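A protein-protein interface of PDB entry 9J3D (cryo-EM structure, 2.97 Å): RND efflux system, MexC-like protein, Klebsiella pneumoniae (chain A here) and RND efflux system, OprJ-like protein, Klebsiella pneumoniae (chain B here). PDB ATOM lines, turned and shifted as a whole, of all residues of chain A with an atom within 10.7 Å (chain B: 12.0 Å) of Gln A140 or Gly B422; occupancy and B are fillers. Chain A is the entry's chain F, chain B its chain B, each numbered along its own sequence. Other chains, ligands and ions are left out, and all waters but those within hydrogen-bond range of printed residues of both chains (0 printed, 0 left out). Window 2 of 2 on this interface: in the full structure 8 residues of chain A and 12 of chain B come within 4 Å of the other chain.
Of the printed residues of chain B, Leu A131 touches Arg B209. No residue of chain B comes within 4 Å of Asp A141. No residue of chain B comes within 4 Å of Asn A144. Ala A145 touches none of the printed residues of chain B. Ala B415 touches none of the printed residues of chain A. Printed residues of chain A within 4 Å of Tyr B419: Asp A135 (3.0 Å). No residue of chain A comes within 4 Å of Gly B421. Of chain A, only Gln A139 (3.2 Å) and Gln A140 (3.1 Å) come within 4 Å of Gly B422. Of the printed residues of chain A, Asp B424 touches Ser A138 (3.9 Å). Printed residues of chain A within 4 Å of Asp B425: Ser A138 (3.9 Å).
Of the 18 printed residues of chain B, 8 touch a printed residue of chain A. Hydrophobic or aromatic side chains of chain B within 4 Å of the printed part of chain A: Tyr B419, Tyr B426 and Leu B427. Hydrophobic or aromatic side chains of chain A within 4 Å of the printed part of chain B: Leu A131 and Ala A136. Among the printed residues, no Asp or Glu carboxylate lies within 4 Å of a Lys or Arg side-chain nitrogen of the other chain.
The backbone carbonyl oxygen (O) of Arg B418 sits at hydrogen-bond distance from the backbone NH (N) of Val B423, at 3.3 Å. The guanidinium group (NE) of Arg B418 lies within salt-bridge range of the side-chain carboxylate (OD2) of Asp B424, at 2.5 Å. The side-chain carboxylate (OD1) of Asp B425 lies within hydrogen-bond range of the backbone NH (N) of Arg B428 (3.1 Å). OG of Ser A138 sits close to N of Gln A140 (3.5 Å). The side-chain hydroxyl (OG) of Ser A138 sits at hydrogen-bond distance from the side-chain carboxylate (OD2) of Asp A141 (2.8 Å). The side-chain amide nitrogen (NE2) of Gln A140 sits at hydrogen-bond distance from the side-chain amide oxygen (OD1) of Asn A144, 3.0 Å away.
The side-chain carboxylate (OD2) of Asp A135 lies close to the side-chain hydroxyl (OH) of Tyr B419, 3.1 Å away. The backbone carbonyl oxygen of Gly B422 lies within hydrogen-bond range of the backbone NH of Gln A139 (3.2 Å). The backbone NH of Gln A140 lies within hydrogen-bond range of the backbone carbonyl oxygen of Gly B422 (3.1 Å).
Among the printed residues, merely in contact across the chains: Leu A131 with Arg B209 (3.95 Å), Asp A135 with Tyr B426 (3.2 Å), Ala A136 with Arg B209 (3.4 Å), Ala A136 with Leu B427 (3.98 Å), Ser A138 with Val B423 (3.4 Å), Ser A138 with Asp B424 (3.9 Å) and Ser A138 with Asp B425 (3.9 Å).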
ATOM      1  N   MET A 124     -20.232   3.849 -10.562  1.00  0.00           N
ATOM      2  CA  MET A 124     -20.152   5.243 -10.137  1.00  0.00           C
ATOM      3  C   MET A 124     -20.424   6.192 -11.298  1.00  0.00           C
ATOM      4  O   MET A 124     -21.184   7.158 -11.159  1.00  0.00           O
ATOM      5  CB  MET A 124     -18.778   5.523  -9.528  1.00  0.00           C
ATOM      6  CG  MET A 124     -18.440   7.000  -9.402  1.00  0.00           C
ATOM      7  SD  MET A 124     -17.557   7.409  -7.887  1.00  0.00           S
ATOM      8  CE  MET A 124     -18.861   7.244  -6.678  1.00  0.00           C
ATOM      9  N   VAL A 125     -19.818   5.926 -12.457  1.00  0.00           N
ATOM     10  CA  VAL A 125     -20.006   6.800 -13.613  1.00  0.00           C
ATOM     11  C   VAL A 125     -21.449   6.739 -14.097  1.00  0.00           C
ATOM     12  O   VAL A 125     -22.046   7.761 -14.457  1.00  0.00           O
ATOM     13  CB  VAL A 125     -19.014   6.432 -14.731  1.00  0.00           C
ATOM     14  CG1 VAL A 125     -19.396   7.115 -16.031  1.00  0.00           C
ATOM     15  CG2 VAL A 125     -17.605   6.816 -14.325  1.00  0.00           C
ATOM     16  N   TYR A 128     -23.497   8.832 -11.750  1.00  0.00           N
ATOM     17  CA  TYR A 128     -23.207  10.261 -11.806  1.00  0.00           C
ATOM     18  C   TYR A 128     -23.622  10.895 -13.128  1.00  0.00           C
ATOM     19  O   TYR A 128     -23.812  12.114 -13.186  1.00  0.00           O
ATOM     20  CB  TYR A 128     -21.717  10.510 -11.562  1.00  0.00           C
ATOM     21  CG  TYR A 128     -21.335  10.597 -10.104  1.00  0.00           C
ATOM     22  CD1 TYR A 128     -22.144  10.053  -9.120  1.00  0.00           C
ATOM     23  CD2 TYR A 128     -20.162  11.224  -9.712  1.00  0.00           C
ATOM     24  CE1 TYR A 128     -21.798  10.130  -7.788  1.00  0.00           C
ATOM     25  CE2 TYR A 128     -19.807  11.307  -8.382  1.00  0.00           C
ATOM     26  CZ  TYR A 128     -20.628  10.759  -7.424  1.00  0.00           C
ATOM     27  OH  TYR A 128     -20.279  10.838  -6.096  1.00  0.00           O
ATOM     28  N   LEU A 131     -26.943  12.667 -12.900  1.00  0.00           N
ATOM     29  CA  LEU A 131     -26.961  13.654 -11.826  1.00  0.00           C
ATOM     30  C   LEU A 131     -26.218  14.923 -12.221  1.00  0.00           C
ATOM     31  O   LEU A 131     -26.588  16.022 -11.793  1.00  0.00           O
ATOM     32  CB  LEU A 131     -26.362  13.057 -10.555  1.00  0.00           C
ATOM     33  CG  LEU A 131     -27.169  11.941  -9.892  1.00  0.00           C
ATOM     34  CD1 LEU A 131     -26.431  11.387  -8.687  1.00  0.00           C
ATOM     35  CD2 LEU A 131     -28.545  12.440  -9.497  1.00  0.00           C
ATOM     36  N   VAL A 132     -25.162  14.798 -13.027  1.00  0.00           N
ATOM     37  CA  VAL A 132     -24.405  15.981 -13.423  1.00  0.00           C
ATOM     38  C   VAL A 132     -25.215  16.850 -14.379  1.00  0.00           C
ATOM     39  O   VAL A 132     -25.038  18.073 -14.416  1.00  0.00           O
ATOM     40  CB  VAL A 132     -23.047  15.573 -14.025  1.00  0.00           C
ATOM     41  CG1 VAL A 132     -23.219  14.987 -15.415  1.00  0.00           C
ATOM     42  CG2 VAL A 132     -22.103  16.761 -14.055  1.00  0.00           C
ATOM     43  N   ASP A 135     -27.210  19.062 -12.340  1.00  0.00           N
ATOM     44  CA  ASP A 135     -26.335  19.778 -11.415  1.00  0.00           C
ATOM     45  C   ASP A 135     -26.400  19.223  -9.997  1.00  0.00           C
ATOM     46  O   ASP A 135     -26.141  19.947  -9.033  1.00  0.00           O
ATOM     47  CB  ASP A 135     -26.644  21.278 -11.410  1.00  0.00           C
ATOM     48  CG  ASP A 135     -26.523  21.898 -12.786  1.00  0.00           C
ATOM     49  OD1 ASP A 135     -25.433  21.803 -13.388  1.00  0.00           O
ATOM     50  OD2 ASP A 135     -27.517  22.480 -13.268  1.00  0.00           O
ATOM     51  N   ALA A 136     -26.739  17.945  -9.849  1.00  0.00           N
ATOM     52  CA  ALA A 136     -26.779  17.318  -8.536  1.00  0.00           C
ATOM     53  C   ALA A 136     -25.396  17.097  -7.944  1.00  0.00           C
ATOM     54  O   ALA A 136     -25.267  17.051  -6.717  1.00  0.00           O
ATOM     55  CB  ALA A 136     -27.524  15.986  -8.616  1.00  0.00           C
ATOM     56  N   VAL A 137     -24.367  16.953  -8.779  1.00  0.00           N
ATOM     57  CA  VAL A 137     -22.990  16.830  -8.323  1.00  0.00           C
ATOM     58  C   VAL A 137     -22.137  17.817  -9.106  1.00  0.00           C
ATOM     59  O   VAL A 137     -22.479  18.225 -10.217  1.00  0.00           O
ATOM     60  CB  VAL A 137     -22.434  15.398  -8.487  1.00  0.00           C
ATOM     61  CG1 VAL A 137     -23.189  14.431  -7.596  1.00  0.00           C
ATOM     62  CG2 VAL A 137     -22.509  14.964  -9.938  1.00  0.00           C
ATOM     63  N   SER A 138     -21.017  18.204  -8.507  1.00  0.00           N
ATOM     64  CA  SER A 138     -20.127  19.159  -9.148  1.00  0.00           C
ATOM     65  C   SER A 138     -19.470  18.539 -10.375  1.00  0.00           C
ATOM     66  O   SER A 138     -19.278  17.324 -10.459  1.00  0.00           O
ATOM     67  CB  SER A 138     -19.060  19.636  -8.167  1.00  0.00           C
ATOM     68  OG  SER A 138     -18.022  18.682  -8.040  1.00  0.00           O
ATOM     69  N   GLN A 139     -19.133  19.396 -11.342  1.00  0.00           N
ATOM     70  CA  GLN A 139     -18.446  18.925 -12.540  1.00  0.00           C
ATOM     71  C   GLN A 139     -17.097  18.311 -12.191  1.00  0.00           C
ATOM     72  O   GLN A 139     -16.644  17.367 -12.851  1.00  0.00           O
ATOM     73  CB  GLN A 139     -18.273  20.080 -13.525  1.00  0.00           C
ATOM     74  CG  GLN A 139     -17.759  19.671 -14.892  1.00  0.00           C
ATOM     75  CD  GLN A 139     -18.773  18.876 -15.683  1.00  0.00           C
ATOM     76  OE1 GLN A 139     -19.971  19.148 -15.624  1.00  0.00           O
ATOM     77  NE2 GLN A 139     -18.298  17.888 -16.432  1.00  0.00           N
ATOM     78  N   GLN A 140     -16.442  18.833 -11.150  1.00  0.00           N
ATOM     79  CA  GLN A 140     -15.167  18.272 -10.718  1.00  0.00           C
ATOM     80  C   GLN A 140     -15.325  16.825 -10.269  1.00  0.00           C
ATOM     81  O   GLN A 140     -14.488  15.972 -10.589  1.00  0.00           O
ATOM     82  CB  GLN A 140     -14.576  19.121  -9.595  1.00  0.00           C
ATOM     83  CG  GLN A 140     -13.233  18.628  -9.103  1.00  0.00           C
ATOM     84  CD  GLN A 140     -12.164  18.712 -10.169  1.00  0.00           C
ATOM     85  OE1 GLN A 140     -11.990  19.747 -10.808  1.00  0.00           O
ATOM     86  NE2 GLN A 140     -11.450  17.612 -10.382  1.00  0.00           N
ATOM     87  N   ASP A 141     -16.390  16.528  -9.524  1.00  0.00           N
ATOM     88  CA  ASP A 141     -16.631  15.157  -9.090  1.00  0.00           C
ATOM     89  C   ASP A 141     -16.879  14.238 -10.280  1.00  0.00           C
ATOM     90  O   ASP A 141     -16.396  13.099 -10.303  1.00  0.00           O
ATOM     91  CB  ASP A 141     -17.811  15.114  -8.123  1.00  0.00           C
ATOM     92  CG  ASP A 141     -17.517  15.822  -6.816  1.00  0.00           C
ATOM     93  OD1 ASP A 141     -16.406  15.639  -6.276  1.00  0.00           O
ATOM     94  OD2 ASP A 141     -18.397  16.562  -6.326  1.00  0.00           O
ATOM     95  N   PHE A 142     -17.634  14.710 -11.272  1.00  0.00           N
ATOM     96  CA  PHE A 142     -17.892  13.898 -12.455  1.00  0.00           C
ATOM     97  C   PHE A 142     -16.604  13.616 -13.217  1.00  0.00           C
ATOM     98  O   PHE A 142     -16.380  12.496 -13.692  1.00  0.00           O
ATOM     99  CB  PHE A 142     -18.911  14.590 -13.355  1.00  0.00           C
ATOM    100  CG  PHE A 142     -19.201  13.844 -14.621  1.00  0.00           C
ATOM    101  CD1 PHE A 142     -19.902  12.652 -14.592  1.00  0.00           C
ATOM    102  CD2 PHE A 142     -18.773  14.333 -15.840  1.00  0.00           C
ATOM    103  CE1 PHE A 142     -20.171  11.963 -15.754  1.00  0.00           C
ATOM    104  CE2 PHE A 142     -19.038  13.649 -17.008  1.00  0.00           C
ATOM    105  CZ  PHE A 142     -19.738  12.462 -16.964  1.00  0.00           C
ATOM    106  N   ASP A 143     -15.742  14.627 -13.348  1.00  0.00           N
ATOM    107  CA  ASP A 143     -14.473  14.414 -14.036  1.00  0.00           C
ATOM    108  C   ASP A 143     -13.573  13.468 -13.252  1.00  0.00           C
ATOM    109  O   ASP A 143     -12.857  12.651 -13.843  1.00  0.00           O
ATOM    110  CB  ASP A 143     -13.777  15.749 -14.284  1.00  0.00           C
ATOM    111  CG  ASP A 143     -14.448  16.556 -15.376  1.00  0.00           C
ATOM    112  OD1 ASP A 143     -15.278  15.983 -16.111  1.00  0.00           O
ATOM    113  OD2 ASP A 143     -14.145  17.760 -15.506  1.00  0.00           O
ATOM    114  N   ASN A 144     -13.594  13.559 -11.921  1.00  0.00           N
ATOM    115  CA  ASN A 144     -12.839  12.613 -11.107  1.00  0.00           C
ATOM    116  C   ASN A 144     -13.343  11.191 -11.312  1.00  0.00           C
ATOM    117  O   ASN A 144     -12.548  10.251 -11.423  1.00  0.00           O
ATOM    118  CB  ASN A 144     -12.921  13.000  -9.632  1.00  0.00           C
ATOM    119  CG  ASN A 144     -12.094  14.223  -9.302  1.00  0.00           C
ATOM    120  OD1 ASN A 144     -11.208  14.611 -10.061  1.00  0.00           O
ATOM    121  ND2 ASN A 144     -12.379  14.839  -8.162  1.00  0.00           N
ATOM    122  N   ALA A 145     -14.665  11.017 -11.366  1.00  0.00           N
ATOM    123  CA  ALA A 145     -15.227   9.692 -11.604  1.00  0.00           C
ATOM    124  C   ALA A 145     -14.839   9.164 -12.979  1.00  0.00           C
ATOM    125  O   ALA A 145     -14.522   7.978 -13.129  1.00  0.00           O
ATOM    126  CB  ALA A 145     -16.746   9.732 -11.454  1.00  0.00           C
ATOM    127  N   MET A 146     -14.863  10.026 -13.995  1.00  0.00           N
ATOM    128  CA  MET A 146     -14.466   9.598 -15.333  1.00  0.00           C
ATOM    129  C   MET A 146     -12.994   9.206 -15.375  1.00  0.00           C
ATOM    130  O   MET A 146     -12.622   8.212 -16.016  1.00  0.00           O
ATOM    131  CB  MET A 146     -14.756  10.704 -16.347  1.00  0.00           C
ATOM    132  CG  MET A 146     -16.198  10.751 -16.820  1.00  0.00           C
ATOM    133  SD  MET A 146     -16.598   9.554 -18.111  1.00  0.00           S
ATOM    134  CE  MET A 146     -14.975   9.126 -18.734  1.00  0.00           C
ATOM    135  N   ALA A 147     -12.140   9.977 -14.702  1.00  0.00           N
ATOM    136  CA  ALA A 147     -10.725   9.633 -14.638  1.00  0.00           C
ATOM    137  C   ALA A 147     -10.519   8.304 -13.928  1.00  0.00           C
ATOM    138  O   ALA A 147      -9.686   7.492 -14.345  1.00  0.00           O
ATOM    139  CB  ALA A 147      -9.945  10.743 -13.938  1.00  0.00           C
ATOM    140  N   ALA A 148     -11.267   8.067 -12.849  1.00  0.00           N
ATOM    141  CA  ALA A 148     -11.173   6.789 -12.154  1.00  0.00           C
ATOM    142  C   ALA A 148     -11.617   5.643 -13.050  1.00  0.00           C
ATOM    143  O   ALA A 148     -11.015   4.565 -13.035  1.00  0.00           O
ATOM    144  CB  ALA A 148     -12.005   6.824 -10.874  1.00  0.00           C
ATOM    145  N   ARG B 209     -31.099  12.973  -6.122  1.00  0.00           N
ATOM    146  CA  ARG B 209     -29.861  12.282  -5.772  1.00  0.00           C
ATOM    147  C   ARG B 209     -30.143  10.952  -5.085  1.00  0.00           C
ATOM    148  O   ARG B 209     -29.485   9.946  -5.371  1.00  0.00           O
ATOM    149  CB  ARG B 209     -28.993  13.164  -4.876  1.00  0.00           C
ATOM    150  CG  ARG B 209     -28.510  14.433  -5.543  1.00  0.00           C
ATOM    151  CD  ARG B 209     -27.149  14.853  -5.026  1.00  0.00           C
ATOM    152  NE  ARG B 209     -26.902  14.368  -3.675  1.00  0.00           N
ATOM    153  CZ  ARG B 209     -25.699  14.251  -3.133  1.00  0.00           C
ATOM    154  NH1 ARG B 209     -24.605  14.572  -3.804  1.00  0.00           N
ATOM    155  NH2 ARG B 209     -25.591  13.802  -1.887  1.00  0.00           N
ATOM    156  N   ALA B 413     -22.072  36.008  -4.227  1.00  0.00           N
ATOM    157  CA  ALA B 413     -21.423  36.228  -5.515  1.00  0.00           C
ATOM    158  C   ALA B 413     -20.291  35.232  -5.729  1.00  0.00           C
ATOM    159  O   ALA B 413     -20.169  34.636  -6.808  1.00  0.00           O
ATOM    160  CB  ALA B 413     -20.906  37.663  -5.610  1.00  0.00           C
ATOM    161  N   LEU B 414     -19.473  35.015  -4.697  1.00  0.00           N
ATOM    162  CA  LEU B 414     -18.369  34.067  -4.817  1.00  0.00           C
ATOM    163  C   LEU B 414     -18.871  32.641  -5.025  1.00  0.00           C
ATOM    164  O   LEU B 414     -18.310  31.894  -5.836  1.00  0.00           O
ATOM    165  CB  LEU B 414     -17.478  34.147  -3.580  1.00  0.00           C
ATOM    166  CG  LEU B 414     -16.668  35.437  -3.465  1.00  0.00           C
ATOM    167  CD1 LEU B 414     -15.989  35.517  -2.115  1.00  0.00           C
ATOM    168  CD2 LEU B 414     -15.650  35.527  -4.583  1.00  0.00           C
ATOM    169  N   ALA B 415     -19.922  32.244  -4.303  1.00  0.00           N
ATOM    170  CA  ALA B 415     -20.457  30.895  -4.458  1.00  0.00           C
ATOM    171  C   ALA B 415     -21.037  30.686  -5.850  1.00  0.00           C
ATOM    172  O   ALA B 415     -20.873  29.616  -6.443  1.00  0.00           O
ATOM    173  CB  ALA B 415     -21.514  30.623  -3.390  1.00  0.00           C
ATOM    174  N   LYS B 416     -21.732  31.694  -6.380  1.00  0.00           N
ATOM    175  CA  LYS B 416     -22.263  31.599  -7.737  1.00  0.00           C
ATOM    176  C   LYS B 416     -21.131  31.483  -8.746  1.00  0.00           C
ATOM    177  O   LYS B 416     -21.208  30.694  -9.695  1.00  0.00           O
ATOM    178  CB  LYS B 416     -23.153  32.814  -8.030  1.00  0.00           C
ATOM    179  CG  LYS B 416     -23.899  32.817  -9.376  1.00  0.00           C
ATOM    180  CD  LYS B 416     -23.030  33.227 -10.561  1.00  0.00           C
ATOM    181  CE  LYS B 416     -23.858  33.449 -11.819  1.00  0.00           C
ATOM    182  NZ  LYS B 416     -24.823  34.572 -11.659  1.00  0.00           N
ATOM    183  N   ALA B 417     -20.068  32.268  -8.558  1.00  0.00           N
ATOM    184  CA  ALA B 417     -18.932  32.191  -9.468  1.00  0.00           C
ATOM    185  C   ALA B 417     -18.291  30.811  -9.430  1.00  0.00           C
ATOM    186  O   ALA B 417     -17.901  30.269 -10.471  1.00  0.00           O
ATOM    187  CB  ALA B 417     -17.911  33.272  -9.123  1.00  0.00           C
ATOM    188  N   ARG B 418     -18.166  30.229  -8.236  1.00  0.00           N
ATOM    189  CA  ARG B 418     -17.616  28.881  -8.130  1.00  0.00           C
ATOM    190  C   ARG B 418     -18.524  27.853  -8.792  1.00  0.00           C
ATOM    191  O   ARG B 418     -18.046  26.974  -9.518  1.00  0.00           O
ATOM    192  CB  ARG B 418     -17.385  28.517  -6.665  1.00  0.00           C
ATOM    193  CG  ARG B 418     -16.206  29.218  -6.029  1.00  0.00           C
ATOM    194  CD  ARG B 418     -16.051  28.811  -4.578  1.00  0.00           C
ATOM    195  NE  ARG B 418     -15.705  27.401  -4.452  1.00  0.00           N
ATOM    196  CZ  ARG B 418     -14.609  26.950  -3.861  1.00  0.00           C
ATOM    197  NH1 ARG B 418     -13.727  27.774  -3.319  1.00  0.00           N
ATOM    198  NH2 ARG B 418     -14.389  25.640  -3.813  1.00  0.00           N
ATOM    199  N   TYR B 419     -19.833  27.940  -8.551  1.00  0.00           N
ATOM    200  CA  TYR B 419     -20.756  26.941  -9.081  1.00  0.00           C
ATOM    201  C   TYR B 419     -20.824  26.996 -10.602  1.00  0.00           C
ATOM    202  O   TYR B 419     -20.843  25.954 -11.268  1.00  0.00           O
ATOM    203  CB  TYR B 419     -22.147  27.128  -8.479  1.00  0.00           C
ATOM    204  CG  TYR B 419     -23.225  26.460  -9.294  1.00  0.00           C
ATOM    205  CD1 TYR B 419     -23.238  25.082  -9.467  1.00  0.00           C
ATOM    206  CD2 TYR B 419     -24.218  27.206  -9.909  1.00  0.00           C
ATOM    207  CE1 TYR B 419     -24.213  24.469 -10.219  1.00  0.00           C
ATOM    208  CE2 TYR B 419     -25.197  26.600 -10.662  1.00  0.00           C
ATOM    209  CZ  TYR B 419     -25.183  25.235 -10.827  1.00  0.00           C
ATOM    210  OH  TYR B 419     -26.168  24.631 -11.572  1.00  0.00           O
ATOM    211  N   GLU B 420     -20.878  28.202 -11.171  1.00  0.00           N
ATOM    212  CA  GLU B 420     -20.922  28.322 -12.624  1.00  0.00           C
ATOM    213  C   GLU B 420     -19.672  27.740 -13.269  1.00  0.00           C
ATOM    214  O   GLU B 420     -19.713  27.308 -14.426  1.00  0.00           O
ATOM    215  CB  GLU B 420     -21.100  29.784 -13.032  1.00  0.00           C
ATOM    216  CG  GLU B 420     -22.549  30.224 -13.201  1.00  0.00           C
ATOM    217  CD  GLU B 420     -23.478  29.082 -13.570  1.00  0.00           C
ATOM    218  OE1 GLU B 420     -24.239  28.628 -12.692  1.00  0.00           O
ATOM    219  OE2 GLU B 420     -23.450  28.641 -14.739  1.00  0.00           O
ATOM    220  N   GLY B 421     -18.558  27.720 -12.543  1.00  0.00           N
ATOM    221  CA  GLY B 421     -17.338  27.103 -13.011  1.00  0.00           C
ATOM    222  C   GLY B 421     -17.265  25.604 -12.838  1.00  0.00           C
ATOM    223  O   GLY B 421     -16.267  24.992 -13.224  1.00  0.00           O
ATOM    224  N   GLY B 422     -18.297  24.991 -12.265  1.00  0.00           N
ATOM    225  CA  GLY B 422     -18.312  23.553 -12.102  1.00  0.00           C
ATOM    226  C   GLY B 422     -17.439  23.022 -10.991  1.00  0.00           C
ATOM    227  O   GLY B 422     -17.097  21.838 -11.000  1.00  0.00           O
ATOM    228  N   VAL B 423     -17.070  23.863 -10.025  1.00  0.00           N
ATOM    229  CA  VAL B 423     -16.222  23.401  -8.932  1.00  0.00           C
ATOM    230  C   VAL B 423     -17.063  22.985  -7.732  1.00  0.00           C
ATOM    231  O   VAL B 423     -16.798  21.955  -7.102  1.00  0.00           O
ATOM    232  CB  VAL B 423     -15.197  24.489  -8.567  1.00  0.00           C
ATOM    233  CG1 VAL B 423     -14.632  24.253  -7.180  1.00  0.00           C
ATOM    234  CG2 VAL B 423     -14.083  24.519  -9.596  1.00  0.00           C
ATOM    235  N   ASP B 424     -18.092  23.760  -7.401  1.00  0.00           N
ATOM    236  CA  ASP B 424     -18.966  23.466  -6.278  1.00  0.00           C
ATOM    237  C   ASP B 424     -20.328  23.008  -6.783  1.00  0.00           C
ATOM    238  O   ASP B 424     -20.781  23.400  -7.861  1.00  0.00           O
ATOM    239  CB  ASP B 424     -19.132  24.684  -5.363  1.00  0.00           C
ATOM    240  CG  ASP B 424     -17.858  25.029  -4.615  1.00  0.00           C
ATOM    241  OD1 ASP B 424     -16.927  24.196  -4.609  1.00  0.00           O
ATOM    242  OD2 ASP B 424     -17.786  26.132  -4.034  1.00  0.00           O
ATOM    243  N   ASP B 425     -20.980  22.169  -5.982  1.00  0.00           N
ATOM    244  CA  ASP B 425     -22.267  21.612  -6.361  1.00  0.00           C
ATOM    245  C   ASP B 425     -23.374  22.655  -6.219  1.00  0.00           C
ATOM    246  O   ASP B 425     -23.162  23.774  -5.745  1.00  0.00           O
ATOM    247  CB  ASP B 425     -22.585  20.377  -5.517  1.00  0.00           C
ATOM    248  CG  ASP B 425     -22.429  20.626  -4.026  1.00  0.00           C
ATOM    249  OD1 ASP B 425     -22.342  21.802  -3.613  1.00  0.00           O
ATOM    250  OD2 ASP B 425     -22.392  19.639  -3.260  1.00  0.00           O
ATOM    251  N   TYR B 426     -24.575  22.267  -6.647  1.00  0.00           N
ATOM    252  CA  TYR B 426     -25.735  23.146  -6.535  1.00  0.00           C
ATOM    253  C   TYR B 426     -26.138  23.374  -5.084  1.00  0.00           C
ATOM    254  O   TYR B 426     -26.711  24.420  -4.759  1.00  0.00           O
ATOM    255  CB  TYR B 426     -26.897  22.553  -7.329  1.00  0.00           C
ATOM    256  CG  TYR B 426     -27.817  23.560  -7.977  1.00  0.00           C
ATOM    257  CD1 TYR B 426     -29.186  23.517  -7.772  1.00  0.00           C
ATOM    258  CD2 TYR B 426     -27.314  24.568  -8.769  1.00  0.00           C
ATOM    259  CE1 TYR B 426     -30.026  24.439  -8.373  1.00  0.00           C
ATOM    260  CE2 TYR B 426     -28.140  25.495  -9.369  1.00  0.00           C
ATOM    261  CZ  TYR B 426     -29.495  25.430  -9.165  1.00  0.00           C
ATOM    262  OH  TYR B 426     -30.320  26.357  -9.760  1.00  0.00           O
ATOM    263  N   LEU B 427     -25.846  22.412  -4.204  1.00  0.00           N
ATOM    264  CA  LEU B 427     -26.236  22.544  -2.806  1.00  0.00           C
ATOM    265  C   LEU B 427     -25.547  23.732  -2.147  1.00  0.00           C
ATOM    266  O   LEU B 427     -26.171  24.466  -1.373  1.00  0.00           O
ATOM    267  CB  LEU B 427     -25.920  21.259  -2.039  1.00  0.00           C
ATOM    268  CG  LEU B 427     -26.738  19.990  -2.315  1.00  0.00           C
ATOM    269  CD1 LEU B 427     -28.229  20.281  -2.266  1.00  0.00           C
ATOM    270  CD2 LEU B 427     -26.345  19.318  -3.623  1.00  0.00           C
ATOM    271  N   ARG B 428     -24.261  23.936  -2.435  1.00  0.00           N
ATOM    272  CA  ARG B 428     -23.542  25.058  -1.838  1.00  0.00           C
ATOM    273  C   ARG B 428     -24.119  26.392  -2.296  1.00  0.00           C
ATOM    274  O   ARG B 428     -24.296  27.312  -1.489  1.00  0.00           O
ATOM    275  CB  ARG B 428     -22.056  24.968  -2.181  1.00  0.00           C
ATOM    276  CG  ARG B 428     -21.198  25.978  -1.443  1.00  0.00           C
ATOM    277  CD  ARG B 428     -21.387  25.850   0.056  1.00  0.00           C
ATOM    278  NE  ARG B 428     -20.601  26.828   0.797  1.00  0.00           N
ATOM    279  CZ  ARG B 428     -20.634  26.965   2.116  1.00  0.00           C
ATOM    280  NH1 ARG B 428     -21.403  26.197   2.871  1.00  0.00           N
ATOM    281  NH2 ARG B 428     -19.881  27.897   2.691  1.00  0.00           N
ATOM    282  N   TYR B 429     -24.425  26.510  -3.588  1.00  0.00           N
ATOM    283  CA  TYR B 429     -25.022  27.737  -4.107  1.00  0.00           C
ATOM    284  C   TYR B 429     -26.390  27.992  -3.484  1.00  0.00           C
ATOM    285  O   TYR B 429     -26.707  29.125  -3.094  1.00  0.00           O
ATOM    286  CB  TYR B 429     -25.119  27.643  -5.630  1.00  0.00           C
ATOM    287  CG  TYR B 429     -25.950  28.712  -6.296  1.00  0.00           C
ATOM    288  CD1 TYR B 429     -25.706  30.056  -6.064  1.00  0.00           C
ATOM    289  CD2 TYR B 429     -26.969  28.374  -7.172  1.00  0.00           C
ATOM    290  CE1 TYR B 429     -26.460  31.030  -6.680  1.00  0.00           C
ATOM    291  CE2 TYR B 429     -27.728  29.342  -7.791  1.00  0.00           C
ATOM    292  CZ  TYR B 429     -27.471  30.669  -7.542  1.00  0.00           C
ATOM    293  OH  TYR B 429     -28.227  31.638  -8.157  1.00  0.00           O
